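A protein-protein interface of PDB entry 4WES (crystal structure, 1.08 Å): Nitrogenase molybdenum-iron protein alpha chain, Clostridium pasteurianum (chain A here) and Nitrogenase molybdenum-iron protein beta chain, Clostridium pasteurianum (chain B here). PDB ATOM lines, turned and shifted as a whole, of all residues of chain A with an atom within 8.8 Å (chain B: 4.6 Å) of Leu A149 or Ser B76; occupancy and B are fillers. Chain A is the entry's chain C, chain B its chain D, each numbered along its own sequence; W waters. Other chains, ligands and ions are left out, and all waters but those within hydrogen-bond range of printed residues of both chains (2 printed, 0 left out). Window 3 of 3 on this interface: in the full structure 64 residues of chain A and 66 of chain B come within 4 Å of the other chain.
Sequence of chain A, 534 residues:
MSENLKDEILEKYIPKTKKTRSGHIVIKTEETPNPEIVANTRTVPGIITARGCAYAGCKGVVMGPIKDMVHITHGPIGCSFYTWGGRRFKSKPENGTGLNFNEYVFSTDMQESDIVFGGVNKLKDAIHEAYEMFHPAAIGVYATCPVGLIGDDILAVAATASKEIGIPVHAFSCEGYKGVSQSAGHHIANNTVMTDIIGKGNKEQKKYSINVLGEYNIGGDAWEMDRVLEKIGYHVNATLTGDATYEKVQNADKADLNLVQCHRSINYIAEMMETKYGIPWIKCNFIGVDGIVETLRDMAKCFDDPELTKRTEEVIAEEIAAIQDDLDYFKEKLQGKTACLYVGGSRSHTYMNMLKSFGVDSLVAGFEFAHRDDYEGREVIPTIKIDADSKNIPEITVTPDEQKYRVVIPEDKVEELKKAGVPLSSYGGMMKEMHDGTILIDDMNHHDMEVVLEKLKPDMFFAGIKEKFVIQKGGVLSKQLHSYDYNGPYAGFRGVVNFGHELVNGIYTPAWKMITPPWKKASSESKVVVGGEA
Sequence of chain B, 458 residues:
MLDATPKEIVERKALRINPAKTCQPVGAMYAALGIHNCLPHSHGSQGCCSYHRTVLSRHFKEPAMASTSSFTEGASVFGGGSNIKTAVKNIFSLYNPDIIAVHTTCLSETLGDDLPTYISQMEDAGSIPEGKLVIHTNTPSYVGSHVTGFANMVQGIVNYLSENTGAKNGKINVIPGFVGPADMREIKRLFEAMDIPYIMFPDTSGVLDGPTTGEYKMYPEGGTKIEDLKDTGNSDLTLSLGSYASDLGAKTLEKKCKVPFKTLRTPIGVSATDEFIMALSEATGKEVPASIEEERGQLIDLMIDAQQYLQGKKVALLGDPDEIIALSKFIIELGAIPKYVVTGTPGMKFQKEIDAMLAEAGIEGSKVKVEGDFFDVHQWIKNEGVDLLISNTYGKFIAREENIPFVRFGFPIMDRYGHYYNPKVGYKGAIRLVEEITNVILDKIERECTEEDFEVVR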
ATOM      1  N   ASP A 114     -38.274  15.819 -16.379  1.00  0.00           N
ATOM      2  CA  ASP A 114     -37.286  14.739 -16.248  1.00  0.00           C
ATOM      3  C   ASP A 114     -35.933  15.292 -15.762  1.00  0.00           C
ATOM      4  O   ASP A 114     -35.224  14.654 -15.017  1.00  0.00           O
ATOM      5  CB  ASP A 114     -37.146  14.000 -17.570  1.00  0.00           C
ATOM      6  CG  ASP A 114     -38.449  13.450 -18.066  1.00  0.00           C
ATOM      7  OD1 ASP A 114     -39.038  12.600 -17.366  1.00  0.00           O
ATOM      8  OD2 ASP A 114     -38.915  13.892 -19.131  1.00  0.00           O
ATOM      9  N   ILE A 115     -35.599  16.515 -16.195  1.00  0.00           N
ATOM     10  CA  ILE A 115     -34.391  17.145 -15.751  1.00  0.00           C
ATOM     11  C   ILE A 115     -34.472  17.458 -14.250  1.00  0.00           C
ATOM     12  O   ILE A 115     -33.519  17.229 -13.499  1.00  0.00           O
ATOM     13  CB  ILE A 115     -34.058  18.407 -16.588  1.00  0.00           C
ATOM     14  CG1 ILE A 115     -33.867  18.017 -18.054  1.00  0.00           C
ATOM     15  CG2 ILE A 115     -32.839  19.136 -16.015  1.00  0.00           C
ATOM     16  CD1 ILE A 115     -32.680  17.125 -18.339  1.00  0.00           C
ATOM     17  N   VAL A 116     -35.597  18.033 -13.821  1.00  0.00           N
ATOM     18  CA  VAL A 116     -35.751  18.462 -12.429  1.00  0.00           C
ATOM     19  C   VAL A 116     -35.862  17.266 -11.471  1.00  0.00           C
ATOM     20  O   VAL A 116     -35.263  17.276 -10.407  1.00  0.00           O
ATOM     21  CB  VAL A 116     -36.955  19.404 -12.253  1.00  0.00           C
ATOM     22  CG1 VAL A 116     -37.213  19.728 -10.794  1.00  0.00           C
ATOM     23  CG2 VAL A 116     -36.757  20.655 -13.094  1.00  0.00           C
ATOM     24  N   GLY A 118     -35.546  13.777 -12.409  1.00  0.00           N
ATOM     25  CA  GLY A 118     -34.984  12.548 -12.902  1.00  0.00           C
ATOM     26  C   GLY A 118     -35.879  11.922 -13.958  1.00  0.00           C
ATOM     27  O   GLY A 118     -37.087  12.187 -14.034  1.00  0.00           O
ATOM     28  N   ALA A 143     -27.185   6.302 -22.362  1.00  0.00           N
ATOM     29  CA  ALA A 143     -27.124   7.619 -21.720  1.00  0.00           C
ATOM     30  C   ALA A 143     -26.688   8.692 -22.692  1.00  0.00           C
ATOM     31  O   ALA A 143     -25.948   8.449 -23.638  1.00  0.00           O
ATOM     32  CB  ALA A 143     -26.180   7.584 -20.544  1.00  0.00           C
ATOM     33  N   THR A 144     -27.138   9.891 -22.413  1.00  0.00           N
ATOM     34  CA  THR A 144     -26.792  11.129 -23.106  1.00  0.00           C
ATOM     35  C   THR A 144     -26.364  12.152 -22.065  1.00  0.00           C
ATOM     36  O   THR A 144     -26.490  11.921 -20.856  1.00  0.00           O
ATOM     37  CB  THR A 144     -27.995  11.630 -23.901  1.00  0.00           C
ATOM     38  OG1 THR A 144     -29.048  11.940 -22.999  1.00  0.00           O
ATOM     39  CG2 THR A 144     -28.453  10.632 -24.963  1.00  0.00           C
ATOM     40  N   CYS A 145     -25.902  13.307 -22.536  1.00  0.00           N
ATOM     41  CA  CYS A 145     -25.371  14.357 -21.643  1.00  0.00           C
ATOM     42  C   CYS A 145     -26.062  14.522 -20.295  1.00  0.00           C
ATOM     43  O   CYS A 145     -25.372  14.550 -19.278  1.00  0.00           O
ATOM     44  CB  CYS A 145     -25.274  15.689 -22.368  1.00  0.00           C
ATOM     45  SG  CYS A 145     -23.903  15.755 -23.567  1.00  0.00           S
ATOM     46  N   PRO A 146     -27.397  14.720 -20.246  1.00  0.00           N
ATOM     47  CA  PRO A 146     -27.973  15.049 -18.923  1.00  0.00           C
ATOM     48  C   PRO A 146     -28.067  13.900 -17.926  1.00  0.00           C
ATOM     49  O   PRO A 146     -28.272  14.133 -16.737  1.00  0.00           O
ATOM     50  CB  PRO A 146     -29.378  15.550 -19.246  1.00  0.00           C
ATOM     51  CG  PRO A 146     -29.604  15.320 -20.663  1.00  0.00           C
ATOM     52  CD  PRO A 146     -28.390  14.843 -21.327  1.00  0.00           C
ATOM     53  N   VAL A 147     -27.985  12.647 -18.408  1.00  0.00           N
ATOM     54  CA  VAL A 147     -28.373  11.487 -17.600  1.00  0.00           C
ATOM     55  C   VAL A 147     -27.616  11.314 -16.272  1.00  0.00           C
ATOM     56  O   VAL A 147     -28.234  11.138 -15.215  1.00  0.00           O
ATOM     57  CB  VAL A 147     -28.304  10.224 -18.461  1.00  0.00           C
ATOM     58  CG1 VAL A 147     -28.548   8.948 -17.617  1.00  0.00           C
ATOM     59  CG2 VAL A 147     -29.338  10.296 -19.565  1.00  0.00           C
ATOM     60  N   GLY A 148     -26.316  11.330 -16.312  1.00  0.00           N
ATOM     61  CA  GLY A 148     -25.552  11.189 -15.088  1.00  0.00           C
ATOM     62  C   GLY A 148     -25.888  12.332 -14.153  1.00  0.00           C
ATOM     63  O   GLY A 148     -26.126  12.135 -12.899  1.00  0.00           O
ATOM     64  N   LEU A 149     -25.895  13.551 -14.715  1.00  0.00           N
ATOM     65  CA  LEU A 149     -26.063  14.772 -13.886  1.00  0.00           C
ATOM     66  C   LEU A 149     -27.382  14.883 -13.140  1.00  0.00           C
ATOM     67  O   LEU A 149     -27.455  15.493 -12.094  1.00  0.00           O
ATOM     68  CB  LEU A 149     -25.858  16.023 -14.752  1.00  0.00           C
ATOM     69  CG  LEU A 149     -24.432  16.117 -15.277  1.00  0.00           C
ATOM     70  CD1 LEU A 149     -24.341  17.065 -16.418  1.00  0.00           C
ATOM     71  CD2 LEU A 149     -23.453  16.489 -14.177  1.00  0.00           C
ATOM     72  N   ILE A 150     -28.416  14.285 -13.684  1.00  0.00           N
ATOM     73  CA  ILE A 150     -29.736  14.375 -13.075  1.00  0.00           C
ATOM     74  C   ILE A 150     -30.014  13.241 -12.091  1.00  0.00           C
ATOM     75  O   ILE A 150     -31.109  13.186 -11.488  1.00  0.00           O
ATOM     76  CB  ILE A 150     -30.862  14.481 -14.094  1.00  0.00           C
ATOM     77  CG1 ILE A 150     -31.014  13.180 -14.853  1.00  0.00           C
ATOM     78  CG2 ILE A 150     -30.640  15.671 -15.010  1.00  0.00           C
ATOM     79  CD1 ILE A 150     -32.098  13.232 -15.900  1.00  0.00           C
ATOM     80  N   GLY A 151     -29.050  12.333 -11.943  1.00  0.00           N
ATOM     81  CA  GLY A 151     -29.123  11.293 -10.918  1.00  0.00           C
ATOM     82  C   GLY A 151     -29.669   9.965 -11.373  1.00  0.00           C
ATOM     83  O   GLY A 151     -29.849   9.099 -10.549  1.00  0.00           O
ATOM     84  N   ASP A 152     -29.925   9.772 -12.657  1.00  0.00           N
ATOM     85  CA  ASP A 152     -30.557   8.525 -13.102  1.00  0.00           C
ATOM     86  C   ASP A 152     -29.597   7.342 -13.056  1.00  0.00           C
ATOM     87  O   ASP A 152     -28.539   7.379 -13.654  1.00  0.00           O
ATOM     88  CB  ASP A 152     -31.049   8.684 -14.540  1.00  0.00           C
ATOM     89  CG  ASP A 152     -32.294   9.527 -14.684  1.00  0.00           C
ATOM     90  OD1 ASP A 152     -32.763  10.142 -13.695  1.00  0.00           O
ATOM     91  OD2 ASP A 152     -32.842   9.593 -15.794  1.00  0.00           O
ATOM     92  N   ASP A 153     -29.978   6.280 -12.367  1.00  0.00           N
ATOM     93  CA  ASP A 153     -29.188   5.025 -12.336  1.00  0.00           C
ATOM     94  C   ASP A 153     -29.746   4.072 -13.385  1.00  0.00           C
ATOM     95  O   ASP A 153     -30.586   3.209 -13.114  1.00  0.00           O
ATOM     96  CB  ASP A 153     -29.218   4.445 -10.941  1.00  0.00           C
ATOM     97  CG  ASP A 153     -28.345   3.217 -10.799  1.00  0.00           C
ATOM     98  OD1 ASP A 153     -27.850   2.712 -11.827  1.00  0.00           O
ATOM     99  OD2 ASP A 153     -28.159   2.786  -9.643  1.00  0.00           O
ATOM    100  N   GLU A 175     -22.676   8.977 -21.806  1.00  0.00           N
ATOM    101  CA  GLU A 175     -22.888  10.418 -21.821  1.00  0.00           C
ATOM    102  C   GLU A 175     -21.873  11.089 -22.725  1.00  0.00           C
ATOM    103  O   GLU A 175     -20.689  10.794 -22.682  1.00  0.00           O
ATOM    104  CB  GLU A 175     -22.782  10.979 -20.408  1.00  0.00           C
ATOM    105  CG  GLU A 175     -23.868  10.586 -19.443  1.00  0.00           C
ATOM    106  CD  GLU A 175     -23.716   9.285 -18.697  1.00  0.00           C
ATOM    107  OE1 GLU A 175     -22.885   8.437 -19.082  1.00  0.00           O
ATOM    108  OE2 GLU A 175     -24.422   9.158 -17.690  1.00  0.00           O
ATOM    109  N   GLY A 176     -22.327  12.091 -23.509  1.00  0.00           N
ATOM    110  CA  GLY A 176     -21.508  12.579 -24.592  1.00  0.00           C
ATOM    111  C   GLY A 176     -20.216  13.261 -24.217  1.00  0.00           C
ATOM    112  O   GLY A 176     -19.284  13.215 -25.010  1.00  0.00           O
ATOM    113  N   TYR A 177     -20.149  13.856 -23.031  1.00  0.00           N
ATOM    114  CA  TYR A 177     -18.940  14.538 -22.570  1.00  0.00           C
ATOM    115  C   TYR A 177     -17.845  13.614 -22.093  1.00  0.00           C
ATOM    116  O   TYR A 177     -16.745  14.064 -21.817  1.00  0.00           O
ATOM    117  CB  TYR A 177     -19.304  15.529 -21.482  1.00  0.00           C
ATOM    118  CG  TYR A 177     -19.997  14.899 -20.283  1.00  0.00           C
ATOM    119  CD1 TYR A 177     -19.284  14.157 -19.344  1.00  0.00           C
ATOM    120  CD2 TYR A 177     -21.376  14.982 -20.142  1.00  0.00           C
ATOM    121  CE1 TYR A 177     -19.909  13.562 -18.272  1.00  0.00           C
ATOM    122  CE2 TYR A 177     -22.012  14.391 -19.060  1.00  0.00           C
ATOM    123  CZ  TYR A 177     -21.274  13.679 -18.149  1.00  0.00           C
ATOM    124  OH  TYR A 177     -21.918  13.105 -17.102  1.00  0.00           O
ATOM    125  N   LYS A 178     -18.135  12.329 -21.967  1.00  0.00           N
ATOM    126  CA  LYS A 178     -17.127  11.371 -21.505  1.00  0.00           C
ATOM    127  C   LYS A 178     -16.055  11.154 -22.553  1.00  0.00           C
ATOM    128  O   LYS A 178     -16.315  11.196 -23.762  1.00  0.00           O
ATOM    129  CB  LYS A 178     -17.769  10.071 -21.066  1.00  0.00           C
ATOM    130  CG  LYS A 178     -18.595  10.300 -19.799  1.00  0.00           C
ATOM    131  CD  LYS A 178     -19.230   9.029 -19.322  1.00  0.00           C
ATOM    132  CE  LYS A 178     -19.886   9.264 -17.985  1.00  0.00           C
ATOM    133  NZ  LYS A 178     -20.622   8.048 -17.521  1.00  0.00           N
ATOM    134  N   ASN A 392     -11.343   8.166 -16.651  1.00  0.00           N
ATOM    135  CA  ASN A 392     -12.483   7.558 -16.005  1.00  0.00           C
ATOM    136  C   ASN A 392     -13.287   6.616 -16.884  1.00  0.00           C
ATOM    137  O   ASN A 392     -14.282   6.094 -16.446  1.00  0.00           O
ATOM    138  CB  ASN A 392     -13.414   8.615 -15.429  1.00  0.00           C
ATOM    139  CG  ASN A 392     -12.760   9.416 -14.342  1.00  0.00           C
ATOM    140  OD1 ASN A 392     -11.981   8.884 -13.540  1.00  0.00           O
ATOM    141  ND2 ASN A 392     -13.047  10.688 -14.319  1.00  0.00           N
ATOM    142  N   THR B  72     -15.687  18.459 -21.707  1.00  0.00           N
ATOM    143  CA  THR B  72     -15.171  17.214 -21.191  1.00  0.00           C
ATOM    144  C   THR B  72     -15.840  16.892 -19.860  1.00  0.00           C
ATOM    145  O   THR B  72     -16.677  17.668 -19.347  1.00  0.00           O
ATOM    146  CB  THR B  72     -13.678  17.320 -20.899  1.00  0.00           C
ATOM    147  OG1 THR B  72     -13.502  18.318 -19.902  1.00  0.00           O
ATOM    148  CG2 THR B  72     -12.886  17.690 -22.162  1.00  0.00           C
ATOM    149  N   GLU B  73     -15.458  15.771 -19.258  1.00  0.00           N
ATOM    150  CA  GLU B  73     -16.026  15.420 -17.970  1.00  0.00           C
ATOM    151  C   GLU B  73     -15.719  16.494 -16.920  1.00  0.00           C
ATOM    152  O   GLU B  73     -16.518  16.778 -16.031  1.00  0.00           O
ATOM    153  CB  GLU B  73     -15.575  14.011 -17.536  1.00  0.00           C
ATOM    154  CG  GLU B  73     -16.287  13.523 -16.277  1.00  0.00           C
ATOM    155  CD  GLU B  73     -16.139  12.032 -16.047  1.00  0.00           C
ATOM    156  OE1 GLU B  73     -15.291  11.425 -16.702  1.00  0.00           O
ATOM    157  OE2 GLU B  73     -16.872  11.492 -15.188  1.00  0.00           O
ATOM    158  N   GLY B  74     -14.562  17.117 -17.033  1.00  0.00           N
ATOM    159  CA  GLY B  74     -14.238  18.210 -16.104  1.00  0.00           C
ATOM    160  C   GLY B  74     -15.244  19.354 -16.148  1.00  0.00           C
ATOM    161  O   GLY B  74     -15.579  19.936 -15.121  1.00  0.00           O
ATOM    162  N   ALA B  75     -15.701  19.697 -17.337  1.00  0.00           N
ATOM    163  CA  ALA B  75     -16.650  20.773 -17.509  1.00  0.00           C
ATOM    164  C   ALA B  75     -17.955  20.381 -16.916  1.00  0.00           C
ATOM    165  O   ALA B  75     -18.741  21.215 -16.483  1.00  0.00           O
ATOM    166  CB  ALA B  75     -16.830  21.087 -18.976  1.00  0.00           C
ATOM    167  N   SER B  76     -18.232  19.087 -16.974  1.00  0.00           N
ATOM    168  CA  SER B  76     -19.487  18.574 -16.440  1.00  0.00           C
ATOM    169  C   SER B  76     -19.515  18.742 -14.927  1.00  0.00           C
ATOM    170  O   SER B  76     -20.574  18.700 -14.317  1.00  0.00           O
ATOM    171  CB  SER B  76     -19.726  17.119 -16.816  1.00  0.00           C
ATOM    172  OG  SER B  76     -18.990  16.237 -15.989  1.00  0.00           O
ATOM    173  N   VAL B  77     -18.345  18.959 -14.341  1.00  0.00           N
ATOM    174  CA  VAL B  77     -18.239  19.265 -12.903  1.00  0.00           C
ATOM    175  C   VAL B  77     -18.098  20.767 -12.587  1.00  0.00           C
ATOM    176  O   VAL B  77     -18.806  21.283 -11.725  1.00  0.00           O
ATOM    177  CB  VAL B  77     -17.059  18.489 -12.291  1.00  0.00           C
ATOM    178  CG1 VAL B  77     -16.825  18.930 -10.862  1.00  0.00           C
ATOM    179  CG2 VAL B  77     -17.315  16.982 -12.360  1.00  0.00           C
ATOM    180  N   PHE B  78     -17.192  21.453 -13.288  1.00  0.00           N
ATOM    181  CA  PHE B  78     -16.827  22.846 -13.026  1.00  0.00           C
ATOM    182  C   PHE B  78     -17.531  23.853 -13.907  1.00  0.00           C
ATOM    183  O   PHE B  78     -17.315  25.070 -13.749  1.00  0.00           O
ATOM    184  CB  PHE B  78     -15.329  23.075 -13.244  1.00  0.00           C
ATOM    185  CG  PHE B  78     -14.482  22.390 -12.247  1.00  0.00           C
ATOM    186  CD1 PHE B  78     -13.784  21.252 -12.562  1.00  0.00           C
ATOM    187  CD2 PHE B  78     -14.389  22.909 -10.960  1.00  0.00           C
ATOM    188  CE1 PHE B  78     -12.996  20.631 -11.611  1.00  0.00           C
ATOM    189  CE2 PHE B  78     -13.603  22.299 -10.005  1.00  0.00           C
ATOM    190  CZ  PHE B  78     -12.903  21.153 -10.328  1.00  0.00           C
ATOM    191  N   LEU B 107     -26.652  19.790 -22.007  1.00  0.00           N
ATOM    192  CA  LEU B 107     -25.575  19.651 -21.009  1.00  0.00           C
ATOM    193  C   LEU B 107     -25.371  20.948 -20.238  1.00  0.00           C
ATOM    194  O   LEU B 107     -25.421  20.977 -19.011  1.00  0.00           O
ATOM    195  CB  LEU B 107     -24.280  19.219 -21.692  1.00  0.00           C
ATOM    196  CG  LEU B 107     -23.077  19.017 -20.774  1.00  0.00           C
ATOM    197  CD1 LEU B 107     -23.373  18.107 -19.615  1.00  0.00           C
ATOM    198  CD2 LEU B 107     -21.906  18.517 -21.608  1.00  0.00           C
ATOM    199  N   THR B 110     -28.480  21.876 -18.192  1.00  0.00           N
ATOM    200  CA  THR B 110     -28.629  21.073 -16.976  1.00  0.00           C
ATOM    201  C   THR B 110     -27.671  21.563 -15.900  1.00  0.00           C
ATOM    202  O   THR B 110     -28.014  21.591 -14.713  1.00  0.00           O
ATOM    203  CB  THR B 110     -28.409  19.568 -17.301  1.00  0.00           C
ATOM    204  OG1 THR B 110     -29.434  19.118 -18.180  1.00  0.00           O
ATOM    205  CG2 THR B 110     -28.417  18.706 -16.058  1.00  0.00           C
ATOM    206  N   LEU B 111     -26.460  21.910 -16.300  1.00  0.00           N
ATOM    207  CA  LEU B 111     -25.436  22.408 -15.400  1.00  0.00           C
ATOM    208  C   LEU B 111     -25.677  23.808 -14.915  1.00  0.00           C
ATOM    209  O   LEU B 111     -25.080  24.218 -13.898  1.00  0.00           O
ATOM    210  CB  LEU B 111     -24.067  22.336 -16.063  1.00  0.00           C
ATOM    211  CG  LEU B 111     -23.468  20.968 -16.307  1.00  0.00           C
ATOM    212  CD1 LEU B 111     -22.284  21.039 -17.274  1.00  0.00           C
ATOM    213  CD2 LEU B 111     -23.072  20.328 -14.982  1.00  0.00           C
HETATM  214  O   HOH W   1     -12.099  10.706 -17.742  1.00  0.00           O
HETATM  215  O   HOH W   2     -13.883  13.781 -20.530  1.00  0.00           O
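The backbone carbonyl oxygen (O) of Tyr A177 lies within hydrogen-bond range of the backbone NH (N) of Glu B73, 3.3 Å away.
ND2 of Asn A392 lies within hydrogen-bond range of OE1 of Glu B73, 3.4 Å away.
Water W2 lies within hydrogen-bond range of the backbone NH of Glu B73 (2.8 Å) and the backbone carbonyl oxygen of Tyr A177 (3.2 Å).
Water W1 bridges N of Asn A392 (2.9 Å) and OE1 of Glu B73 (3.4 Å).
Among the printed residues, pairs that only touch across the chains: Leu A149 with Leu B107 (3.5 Å), Tyr A177 with Thr B72 (3.6 Å), Leu A149 with Ser B76 (3.6 Å), Tyr A177 with Ser B76 (3.6 Å), Pro A146 with Thr B110 (3.7 Å), Cys A145 with Leu B107 (3.7 Å), Tyr A177 with Leu B107 (3.7 Å), Leu A149 with Leu B111 (3.8 Å), Ile A115 with Thr B110 (3.8 Å), Ile A150 with Thr B110 (3.9 Å) and Leu A149 with Thr B110 (3.9 Å).
O of Glu B73 sits at hydrogen-bond distance from OG of Ser B76, 2.5 Å away.
N of Gly B74 lies close to OG1 of Thr B72 (3.3 Å).
Of the printed residues of chain B, Pro A146 touches Thr B110 (3.7 Å).
Of the printed residues of chain B, Leu A149 touches Ser B76 (3.6 Å), Leu B107 (3.5 Å), Thr B110 (3.9 Å) and Leu B111 (3.8 Å).
No residue of chain A comes within 4 Å of Gly B74.
Ser B76 touches two residues of chain A.
Of the printed residues of chain A, Thr B110 touches Ile A115, Pro A146, Leu A149 and Ile A150.
The nearest printed residue of chain B that does not touch Cys A145 is Thr B110 (6.1 Å).
Printed residues of chain A that touch a printed residue of chain B: Ile A115, Cys A145, Pro A146, Leu A149, Ile A150, Tyr A177 and Asn A392.
Hydrophobic or aromatic side chains of chain A that line the printed part of chain B: Ile A115, Pro A146, Leu A149, Ile A150 and Tyr A177.
Printed residues of chain B that touch a printed residue of chain A: Thr B72, Glu B73, Ser B76, Leu B107, Thr B110 and Leu B111.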
